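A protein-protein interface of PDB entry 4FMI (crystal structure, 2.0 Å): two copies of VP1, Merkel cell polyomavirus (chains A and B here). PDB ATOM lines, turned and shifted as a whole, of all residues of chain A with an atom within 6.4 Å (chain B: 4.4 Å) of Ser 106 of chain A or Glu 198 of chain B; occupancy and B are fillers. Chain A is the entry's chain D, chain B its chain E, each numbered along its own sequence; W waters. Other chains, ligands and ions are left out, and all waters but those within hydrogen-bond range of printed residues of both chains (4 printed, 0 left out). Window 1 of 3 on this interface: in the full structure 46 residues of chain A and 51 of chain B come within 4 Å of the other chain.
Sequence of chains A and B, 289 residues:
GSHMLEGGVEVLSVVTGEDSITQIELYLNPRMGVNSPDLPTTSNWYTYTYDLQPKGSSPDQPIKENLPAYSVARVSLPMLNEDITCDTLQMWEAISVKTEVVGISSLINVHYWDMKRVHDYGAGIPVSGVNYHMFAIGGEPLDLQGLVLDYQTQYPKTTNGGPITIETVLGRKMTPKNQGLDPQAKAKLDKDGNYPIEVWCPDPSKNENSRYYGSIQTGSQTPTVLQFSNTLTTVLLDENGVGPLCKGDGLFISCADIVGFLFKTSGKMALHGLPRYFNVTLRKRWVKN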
ATOM      1  N   VAL A 102     -15.498   4.694   9.126  1.00  0.00           N
ATOM      2  CA  VAL A 102     -16.737   3.952   9.327  1.00  0.00           C
ATOM      3  C   VAL A 102     -16.531   2.492   8.889  1.00  0.00           C
ATOM      4  O   VAL A 102     -15.782   2.222   7.946  1.00  0.00           O
ATOM      5  CB  VAL A 102     -17.896   4.650   8.541  1.00  0.00           C
ATOM      6  CG1 VAL A 102     -19.147   3.800   8.464  1.00  0.00           C
ATOM      7  CG2 VAL A 102     -18.210   6.006   9.168  1.00  0.00           C
ATOM      8  N   GLY A 103     -17.164   1.557   9.595  1.00  0.00           N
ATOM      9  CA  GLY A 103     -17.121   0.144   9.211  1.00  0.00           C
ATOM     10  C   GLY A 103     -15.876  -0.622   9.639  1.00  0.00           C
ATOM     11  O   GLY A 103     -15.590  -1.691   9.104  1.00  0.00           O
ATOM     12  N   ILE A 104     -15.131  -0.072  10.596  1.00  0.00           N
ATOM     13  CA  ILE A 104     -13.884  -0.687  11.072  1.00  0.00           C
ATOM     14  C   ILE A 104     -14.164  -2.105  11.566  1.00  0.00           C
ATOM     15  O   ILE A 104     -13.413  -3.030  11.271  1.00  0.00           O
ATOM     16  CB  ILE A 104     -13.179   0.204  12.155  1.00  0.00           C
ATOM     17  CG1 ILE A 104     -12.530   1.433  11.492  1.00  0.00           C
ATOM     18  CG2 ILE A 104     -12.140  -0.583  12.959  1.00  0.00           C
ATOM     19  CD1 ILE A 104     -11.969   2.487  12.472  1.00  0.00           C
ATOM     20  N   SER A 105     -15.297  -2.277  12.252  1.00  0.00           N
ATOM     21  CA  SER A 105     -15.674  -3.553  12.843  1.00  0.00           C
ATOM     22  C   SER A 105     -15.846  -4.689  11.824  1.00  0.00           C
ATOM     23  O   SER A 105     -15.670  -5.848  12.162  1.00  0.00           O
ATOM     24  CB  SER A 105     -16.954  -3.381  13.678  1.00  0.00           C
ATOM     25  OG  SER A 105     -18.098  -3.166  12.856  1.00  0.00           O
ATOM     26  N   SER A 106     -16.181  -4.352  10.579  1.00  0.00           N
ATOM     27  CA  SER A 106     -16.386  -5.361   9.545  1.00  0.00           C
ATOM     28  C   SER A 106     -15.128  -6.174   9.298  1.00  0.00           C
ATOM     29  O   SER A 106     -15.201  -7.288   8.780  1.00  0.00           O
ATOM     30  CB  SER A 106     -16.850  -4.727   8.236  1.00  0.00           C
ATOM     31  OG  SER A 106     -15.860  -3.861   7.723  1.00  0.00           O
ATOM     32  N   LEU A 107     -13.983  -5.610   9.675  1.00  0.00           N
ATOM     33  CA  LEU A 107     -12.689  -6.247   9.444  1.00  0.00           C
ATOM     34  C   LEU A 107     -12.352  -7.419  10.390  1.00  0.00           C
ATOM     35  O   LEU A 107     -11.293  -8.034  10.233  1.00  0.00           O
ATOM     36  CB  LEU A 107     -11.557  -5.200   9.458  1.00  0.00           C
ATOM     37  CG  LEU A 107     -11.650  -3.985   8.529  1.00  0.00           C
ATOM     38  CD1 LEU A 107     -10.349  -3.151   8.562  1.00  0.00           C
ATOM     39  CD2 LEU A 107     -11.974  -4.421   7.104  1.00  0.00           C
ATOM     40  N   ILE A 108     -13.230  -7.722  11.355  1.00  0.00           N
ATOM     41  CA  ILE A 108     -13.068  -8.938  12.173  1.00  0.00           C
ATOM     42  C   ILE A 108     -13.469 -10.222  11.424  1.00  0.00           C
ATOM     43  O   ILE A 108     -13.165 -11.321  11.882  1.00  0.00           O
ATOM     44  CB  ILE A 108     -13.805  -8.890  13.545  1.00  0.00           C
ATOM     45  CG1 ILE A 108     -15.324  -8.974  13.373  1.00  0.00           C
ATOM     46  CG2 ILE A 108     -13.370  -7.670  14.368  1.00  0.00           C
ATOM     47  CD1 ILE A 108     -16.054  -9.541  14.615  1.00  0.00           C
ATOM     48  N   ASN A 109     -14.147 -10.059  10.283  1.00  0.00           N
ATOM     49  CA  ASN A 109     -14.558 -11.159   9.408  1.00  0.00           C
ATOM     50  C   ASN A 109     -13.347 -11.922   8.887  1.00  0.00           C
ATOM     51  O   ASN A 109     -12.589 -11.412   8.063  1.00  0.00           O
ATOM     52  CB  ASN A 109     -15.389 -10.605   8.237  1.00  0.00           C
ATOM     53  CG  ASN A 109     -15.949 -11.694   7.324  1.00  0.00           C
ATOM     54  OD1 ASN A 109     -15.539 -12.854   7.386  1.00  0.00           O
ATOM     55  ND2 ASN A 109     -16.892 -11.311   6.460  1.00  0.00           N
ATOM     56  N   VAL A 110     -13.164 -13.141   9.389  1.00  0.00           N
ATOM     57  CA  VAL A 110     -12.061 -14.005   8.954  1.00  0.00           C
ATOM     58  C   VAL A 110     -12.590 -15.242   8.220  1.00  0.00           C
ATOM     59  O   VAL A 110     -11.947 -16.287   8.203  1.00  0.00           O
ATOM     60  CB  VAL A 110     -11.105 -14.396  10.142  1.00  0.00           C
ATOM     61  CG1 VAL A 110     -10.371 -13.159  10.657  1.00  0.00           C
ATOM     62  CG2 VAL A 110     -11.863 -15.069  11.274  1.00  0.00           C
ATOM     63  N   HIS A 111     -13.758 -15.096   7.597  1.00  0.00           N
ATOM     64  CA  HIS A 111     -14.459 -16.218   6.963  1.00  0.00           C
ATOM     65  C   HIS A 111     -15.107 -15.786   5.643  1.00  0.00           C
ATOM     66  O   HIS A 111     -16.202 -16.228   5.288  1.00  0.00           O
ATOM     67  CB  HIS A 111     -15.496 -16.813   7.917  1.00  0.00           C
ATOM     68  CG  HIS A 111     -16.500 -15.815   8.390  1.00  0.00           C
ATOM     69  ND1 HIS A 111     -17.651 -15.532   7.688  1.00  0.00           N
ATOM     70  CD2 HIS A 111     -16.502 -14.996   9.468  1.00  0.00           C
ATOM     71  CE1 HIS A 111     -18.333 -14.598   8.327  1.00  0.00           C
ATOM     72  NE2 HIS A 111     -17.659 -14.258   9.412  1.00  0.00           N
ATOM     73  N   HIS A 272      -8.273  -3.032   0.074  1.00  0.00           N
ATOM     74  CA  HIS A 272      -9.637  -2.743   0.515  1.00  0.00           C
ATOM     75  C   HIS A 272      -9.624  -1.368   1.185  1.00  0.00           C
ATOM     76  O   HIS A 272      -8.621  -0.986   1.812  1.00  0.00           O
ATOM     77  CB  HIS A 272     -10.091  -3.842   1.478  1.00  0.00           C
ATOM     78  CG  HIS A 272     -11.471  -3.672   2.032  1.00  0.00           C
ATOM     79  ND1 HIS A 272     -12.553  -3.295   1.264  1.00  0.00           N
ATOM     80  CD2 HIS A 272     -11.960  -3.911   3.276  1.00  0.00           C
ATOM     81  CE1 HIS A 272     -13.641  -3.275   2.016  1.00  0.00           C
ATOM     82  NE2 HIS A 272     -13.310  -3.643   3.242  1.00  0.00           N
ATOM     83  N   LEU A 274     -12.196   1.790   3.370  1.00  0.00           N
ATOM     84  CA  LEU A 274     -13.379   2.069   4.198  1.00  0.00           C
ATOM     85  C   LEU A 274     -13.823   3.526   4.031  1.00  0.00           C
ATOM     86  O   LEU A 274     -12.999   4.378   3.663  1.00  0.00           O
ATOM     87  CB  LEU A 274     -13.111   1.764   5.678  1.00  0.00           C
ATOM     88  CG  LEU A 274     -13.112   0.301   6.137  1.00  0.00           C
ATOM     89  CD1 LEU A 274     -12.801   0.223   7.621  1.00  0.00           C
ATOM     90  CD2 LEU A 274     -14.455  -0.370   5.847  1.00  0.00           C
ATOM     91  N   LEU B  67     -20.618 -15.614  14.961  1.00  0.00           N
ATOM     92  CA  LEU B  67     -20.831 -14.171  14.890  1.00  0.00           C
ATOM     93  C   LEU B  67     -20.790 -13.501  16.278  1.00  0.00           C
ATOM     94  O   LEU B  67     -21.833 -13.360  16.940  1.00  0.00           O
ATOM     95  CB  LEU B  67     -22.148 -13.871  14.151  1.00  0.00           C
ATOM     96  CG  LEU B  67     -22.271 -14.427  12.719  1.00  0.00           C
ATOM     97  CD1 LEU B  67     -23.717 -14.366  12.232  1.00  0.00           C
ATOM     98  CD2 LEU B  67     -21.320 -13.715  11.735  1.00  0.00           C
ATOM     99  N   LEU B 147     -22.277  -2.089   7.802  1.00  0.00           N
ATOM    100  CA  LEU B 147     -21.250  -2.227   6.747  1.00  0.00           C
ATOM    101  C   LEU B 147     -20.553  -3.576   6.906  1.00  0.00           C
ATOM    102  O   LEU B 147     -20.025  -3.887   7.983  1.00  0.00           O
ATOM    103  CB  LEU B 147     -20.219  -1.112   6.831  1.00  0.00           C
ATOM    104  CG  LEU B 147     -19.177  -0.948   5.715  1.00  0.00           C
ATOM    105  CD1 LEU B 147     -18.732   0.508   5.676  1.00  0.00           C
ATOM    106  CD2 LEU B 147     -17.973  -1.896   5.871  1.00  0.00           C
ATOM    107  N   VAL B 148     -20.548  -4.356   5.827  1.00  0.00           N
ATOM    108  CA  VAL B 148     -20.008  -5.717   5.818  1.00  0.00           C
ATOM    109  C   VAL B 148     -18.882  -5.840   4.784  1.00  0.00           C
ATOM    110  O   VAL B 148     -18.865  -5.112   3.788  1.00  0.00           O
ATOM    111  CB  VAL B 148     -21.114  -6.755   5.517  1.00  0.00           C
ATOM    112  CG1 VAL B 148     -22.192  -6.729   6.600  1.00  0.00           C
ATOM    113  CG2 VAL B 148     -21.736  -6.527   4.112  1.00  0.00           C
ATOM    114  N   LEU B 149     -17.945  -6.751   5.041  1.00  0.00           N
ATOM    115  CA  LEU B 149     -16.856  -7.092   4.113  1.00  0.00           C
ATOM    116  C   LEU B 149     -17.365  -7.571   2.746  1.00  0.00           C
ATOM    117  O   LEU B 149     -16.797  -7.226   1.702  1.00  0.00           O
ATOM    118  CB  LEU B 149     -15.960  -8.181   4.733  1.00  0.00           C
ATOM    119  CG  LEU B 149     -14.633  -8.571   4.060  1.00  0.00           C
ATOM    120  CD1 LEU B 149     -13.556  -7.500   4.278  1.00  0.00           C
ATOM    121  CD2 LEU B 149     -14.127  -9.901   4.593  1.00  0.00           C
ATOM    122  N   TYR B 155     -26.348 -14.114   6.022  1.00  0.00           N
ATOM    123  CA  TYR B 155     -26.421 -14.228   7.480  1.00  0.00           C
ATOM    124  C   TYR B 155     -27.653 -15.020   7.887  1.00  0.00           C
ATOM    125  O   TYR B 155     -28.614 -15.094   7.124  1.00  0.00           O
ATOM    126  CB  TYR B 155     -26.418 -12.834   8.122  1.00  0.00           C
ATOM    127  CG  TYR B 155     -25.078 -12.152   7.970  1.00  0.00           C
ATOM    128  CD1 TYR B 155     -24.031 -12.429   8.855  1.00  0.00           C
ATOM    129  CD2 TYR B 155     -24.836 -11.266   6.920  1.00  0.00           C
ATOM    130  CE1 TYR B 155     -22.792 -11.825   8.713  1.00  0.00           C
ATOM    131  CE2 TYR B 155     -23.592 -10.656   6.771  1.00  0.00           C
ATOM    132  CZ  TYR B 155     -22.582 -10.944   7.673  1.00  0.00           C
ATOM    133  OH  TYR B 155     -21.354 -10.359   7.533  1.00  0.00           O
ATOM    134  N   PRO B 196     -24.357  -8.603  15.326  1.00  0.00           N
ATOM    135  CA  PRO B 196     -23.016  -9.050  14.989  1.00  0.00           C
ATOM    136  C   PRO B 196     -22.050  -7.903  14.821  1.00  0.00           C
ATOM    137  O   PRO B 196     -22.343  -6.944  14.111  1.00  0.00           O
ATOM    138  CB  PRO B 196     -23.216  -9.757  13.652  1.00  0.00           C
ATOM    139  CG  PRO B 196     -24.604 -10.292  13.745  1.00  0.00           C
ATOM    140  CD  PRO B 196     -25.361  -9.175  14.412  1.00  0.00           C
ATOM    141  N   ILE B 197     -20.905  -8.022  15.481  1.00  0.00           N
ATOM    142  CA  ILE B 197     -19.836  -7.036  15.401  1.00  0.00           C
ATOM    143  C   ILE B 197     -19.356  -6.830  13.952  1.00  0.00           C
ATOM    144  O   ILE B 197     -19.109  -5.692  13.536  1.00  0.00           O
ATOM    145  CB  ILE B 197     -18.660  -7.413  16.358  1.00  0.00           C
ATOM    146  CG1 ILE B 197     -19.071  -7.187  17.817  1.00  0.00           C
ATOM    147  CG2 ILE B 197     -17.387  -6.607  16.038  1.00  0.00           C
ATOM    148  CD1 ILE B 197     -18.170  -7.862  18.830  1.00  0.00           C
ATOM    149  N   GLU B 198     -19.264  -7.914  13.181  1.00  0.00           N
ATOM    150  CA  GLU B 198     -18.772  -7.828  11.798  1.00  0.00           C
ATOM    151  C   GLU B 198     -19.763  -7.126  10.856  1.00  0.00           C
ATOM    152  O   GLU B 198     -19.412  -6.759   9.742  1.00  0.00           O
ATOM    153  CB  GLU B 198     -18.389  -9.216  11.254  1.00  0.00           C
ATOM    154  CG  GLU B 198     -19.527 -10.030  10.647  1.00  0.00           C
ATOM    155  CD  GLU B 198     -19.063 -11.350  10.039  1.00  0.00           C
ATOM    156  OE1 GLU B 198     -18.213 -12.040  10.650  1.00  0.00           O
ATOM    157  OE2 GLU B 198     -19.561 -11.702   8.944  1.00  0.00           O
ATOM    158  N   VAL B 199     -20.999  -6.940  11.317  1.00  0.00           N
ATOM    159  CA  VAL B 199     -22.021  -6.267  10.511  1.00  0.00           C
ATOM    160  C   VAL B 199     -22.220  -4.797  10.928  1.00  0.00           C
ATOM    161  O   VAL B 199     -22.410  -3.922  10.081  1.00  0.00           O
ATOM    162  CB  VAL B 199     -23.356  -7.062  10.539  1.00  0.00           C
ATOM    163  CG1 VAL B 199     -24.476  -6.292   9.854  1.00  0.00           C
ATOM    164  CG2 VAL B 199     -23.166  -8.418   9.885  1.00  0.00           C
ATOM    165  N   TRP B 200     -22.134  -4.533  12.230  1.00  0.00           N
ATOM    166  CA  TRP B 200     -22.495  -3.229  12.791  1.00  0.00           C
ATOM    167  C   TRP B 200     -21.310  -2.515  13.448  1.00  0.00           C
ATOM    168  O   TRP B 200     -20.472  -3.149  14.087  1.00  0.00           O
ATOM    169  CB  TRP B 200     -23.634  -3.404  13.810  1.00  0.00           C
ATOM    170  CG  TRP B 200     -24.862  -4.045  13.237  1.00  0.00           C
ATOM    171  CD1 TRP B 200     -25.261  -5.340  13.399  1.00  0.00           C
ATOM    172  CD2 TRP B 200     -25.850  -3.420  12.394  1.00  0.00           C
ATOM    173  NE1 TRP B 200     -26.434  -5.559  12.720  1.00  0.00           N
ATOM    174  CE2 TRP B 200     -26.817  -4.400  12.092  1.00  0.00           C
ATOM    175  CE3 TRP B 200     -26.007  -2.126  11.869  1.00  0.00           C
ATOM    176  CZ2 TRP B 200     -27.933  -4.132  11.287  1.00  0.00           C
ATOM    177  CZ3 TRP B 200     -27.113  -1.854  11.066  1.00  0.00           C
ATOM    178  CH2 TRP B 200     -28.065  -2.857  10.785  1.00  0.00           C
HETATM  179  O   HOH W   1     -19.191  -2.386  10.107  1.00  0.00           O
HETATM  180  O   HOH W   2     -19.443  -9.750   5.510  1.00  0.00           O
HETATM  181  O   HOH W   3     -16.777  -3.776   2.913  1.00  0.00           O
HETATM  182  O   HOH W   4     -17.939  -8.242   7.917  1.00  0.00           O
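O of Ile 197 of chain B is in hydrogen-bond range of OG of Ser 105 of chain A, 2.8 Å away.
OG of Ser 105 of chain A lies within hydrogen-bond range of O of Trp 200 of chain B, 2.7 Å away.
A ring nitrogen (NE2) of His 111 of chain A sits at hydrogen-bond distance from the side-chain carboxylate of Glu 198 of chain B (2.6 Å).
The backbone carbonyl oxygen of Gly 103 of chain A lies within hydrogen-bond range of the side-chain hydroxyl of Ser 106 of chain A, at 2.6 Å.
The backbone NH (N) of His 111 of chain A is in hydrogen-bond range of the side-chain amide oxygen (OD1) of Asn 109 of chain A (2.9 Å).
The backbone NH (N) of Leu 147 of chain B sits at hydrogen-bond distance from the backbone carbonyl oxygen (O) of Val 199 of chain B (2.9 Å).
OH of Tyr 155 of chain B is in hydrogen-bond range of OE2 of Glu 198 of chain B (2.6 Å).
Among the printed residues, merely in contact across the chains: Ser 106 of chain A with Leu 147 of chain B (3.3 Å), Ser 106 of chain A with Glu 198 of chain B (3.3 Å), Ile 108 of chain A with Ile 197 of chain B (3.5 Å), Asn 109 of chain A with Leu 149 of chain B (3.6 Å), Asn 109 of chain A with Glu 198 of chain B (3.7 Å), Ser 105 of chain A with Glu 198 of chain B (3.7 Å), Ile 108 of chain A with Glu 198 of chain B (3.7 Å), Leu 274 of chain A with Leu 147 of chain B (3.8 Å), Gly 103 of chain A with Leu 147 of chain B (3.9 Å) and Ser 106 of chain A with Leu 149 of chain B (3.9 Å).
Ser 106 of chain A touches just these residues of chain B: Leu 147 (3.3 Å), Leu 149 (3.9 Å) and Glu 198 (3.3 Å).
Glu 198 of chain B touches just these residues of chain A: Ser 105 (3.7 Å), Ser 106 (3.3 Å), Ile 108 (3.7 Å), Asn 109 (3.7 Å) and His 111 (2.6 Å).
Of the printed residues of chain A, Trp 200 of chain B touches Ser 105.
Printed residues of chain A within 4 Å of Leu 147 of chain B: Gly 103 (3.9 Å), Ser 106 (3.3 Å) and Leu 274 (3.8 Å).
Of the printed residues of chain A, Leu 149 of chain B touches Ser 106 (3.9 Å) and Asn 109 (3.6 Å).
Printed residues of chain A within 4 Å of Ile 197 of chain B: Ser 105 and Ile 108.
Of the 10 printed residues of chain B, 5 touch a printed residue of chain A.
Printed residues of chain B that touch a printed residue of chain A: Leu 147, Leu 149, Ile 197, Glu 198 and Trp 200.
Hydrophobic or aromatic side chains of chain B within 4 Å of the printed part of chain A: Leu 147, Leu 149 and Ile 197.
Printed residues of chain A that touch a printed residue of chain B: Gly 103, Ser 105, Ser 106, Ile 108, Asn 109, His 111 and Leu 274.
Hydrophobic or aromatic side chains of chain A that line the printed part of chain B: Ile 108, His 111 and Leu 274.
Among the printed residues, no Asp or Glu carboxylate lies within 4 Å of a Lys or Arg side-chain nitrogen of the other chain.
No position is printed for both chains.
Of the 13 pairs that touch across the chains among the printed residues, none has its exchanged pair printed and touching as well.
Water W3 bridges O of Val 148 of chain B (2.6 Å) and NE2 of His 272 of chain A (3.5 Å).
Water W1 bridges the backbone carbonyl oxygen of Leu 147 of chain B (2.7 Å) and the side-chain hydroxyl of Ser 105 of chain A (3.1 Å).
Water W4 lies within hydrogen-bond range of O of Glu 198 of chain B (2.8 Å), O of Ser 106 of chain A (3.0 Å) and N of Leu 149 of chain B (3.2 Å).
Water W2 lies within hydrogen-bond range of OH of Tyr 155 of chain B (2.8 Å), ND2 of Asn 109 of chain A (3.1 Å) and N of Leu 149 of chain B (3.4 Å).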
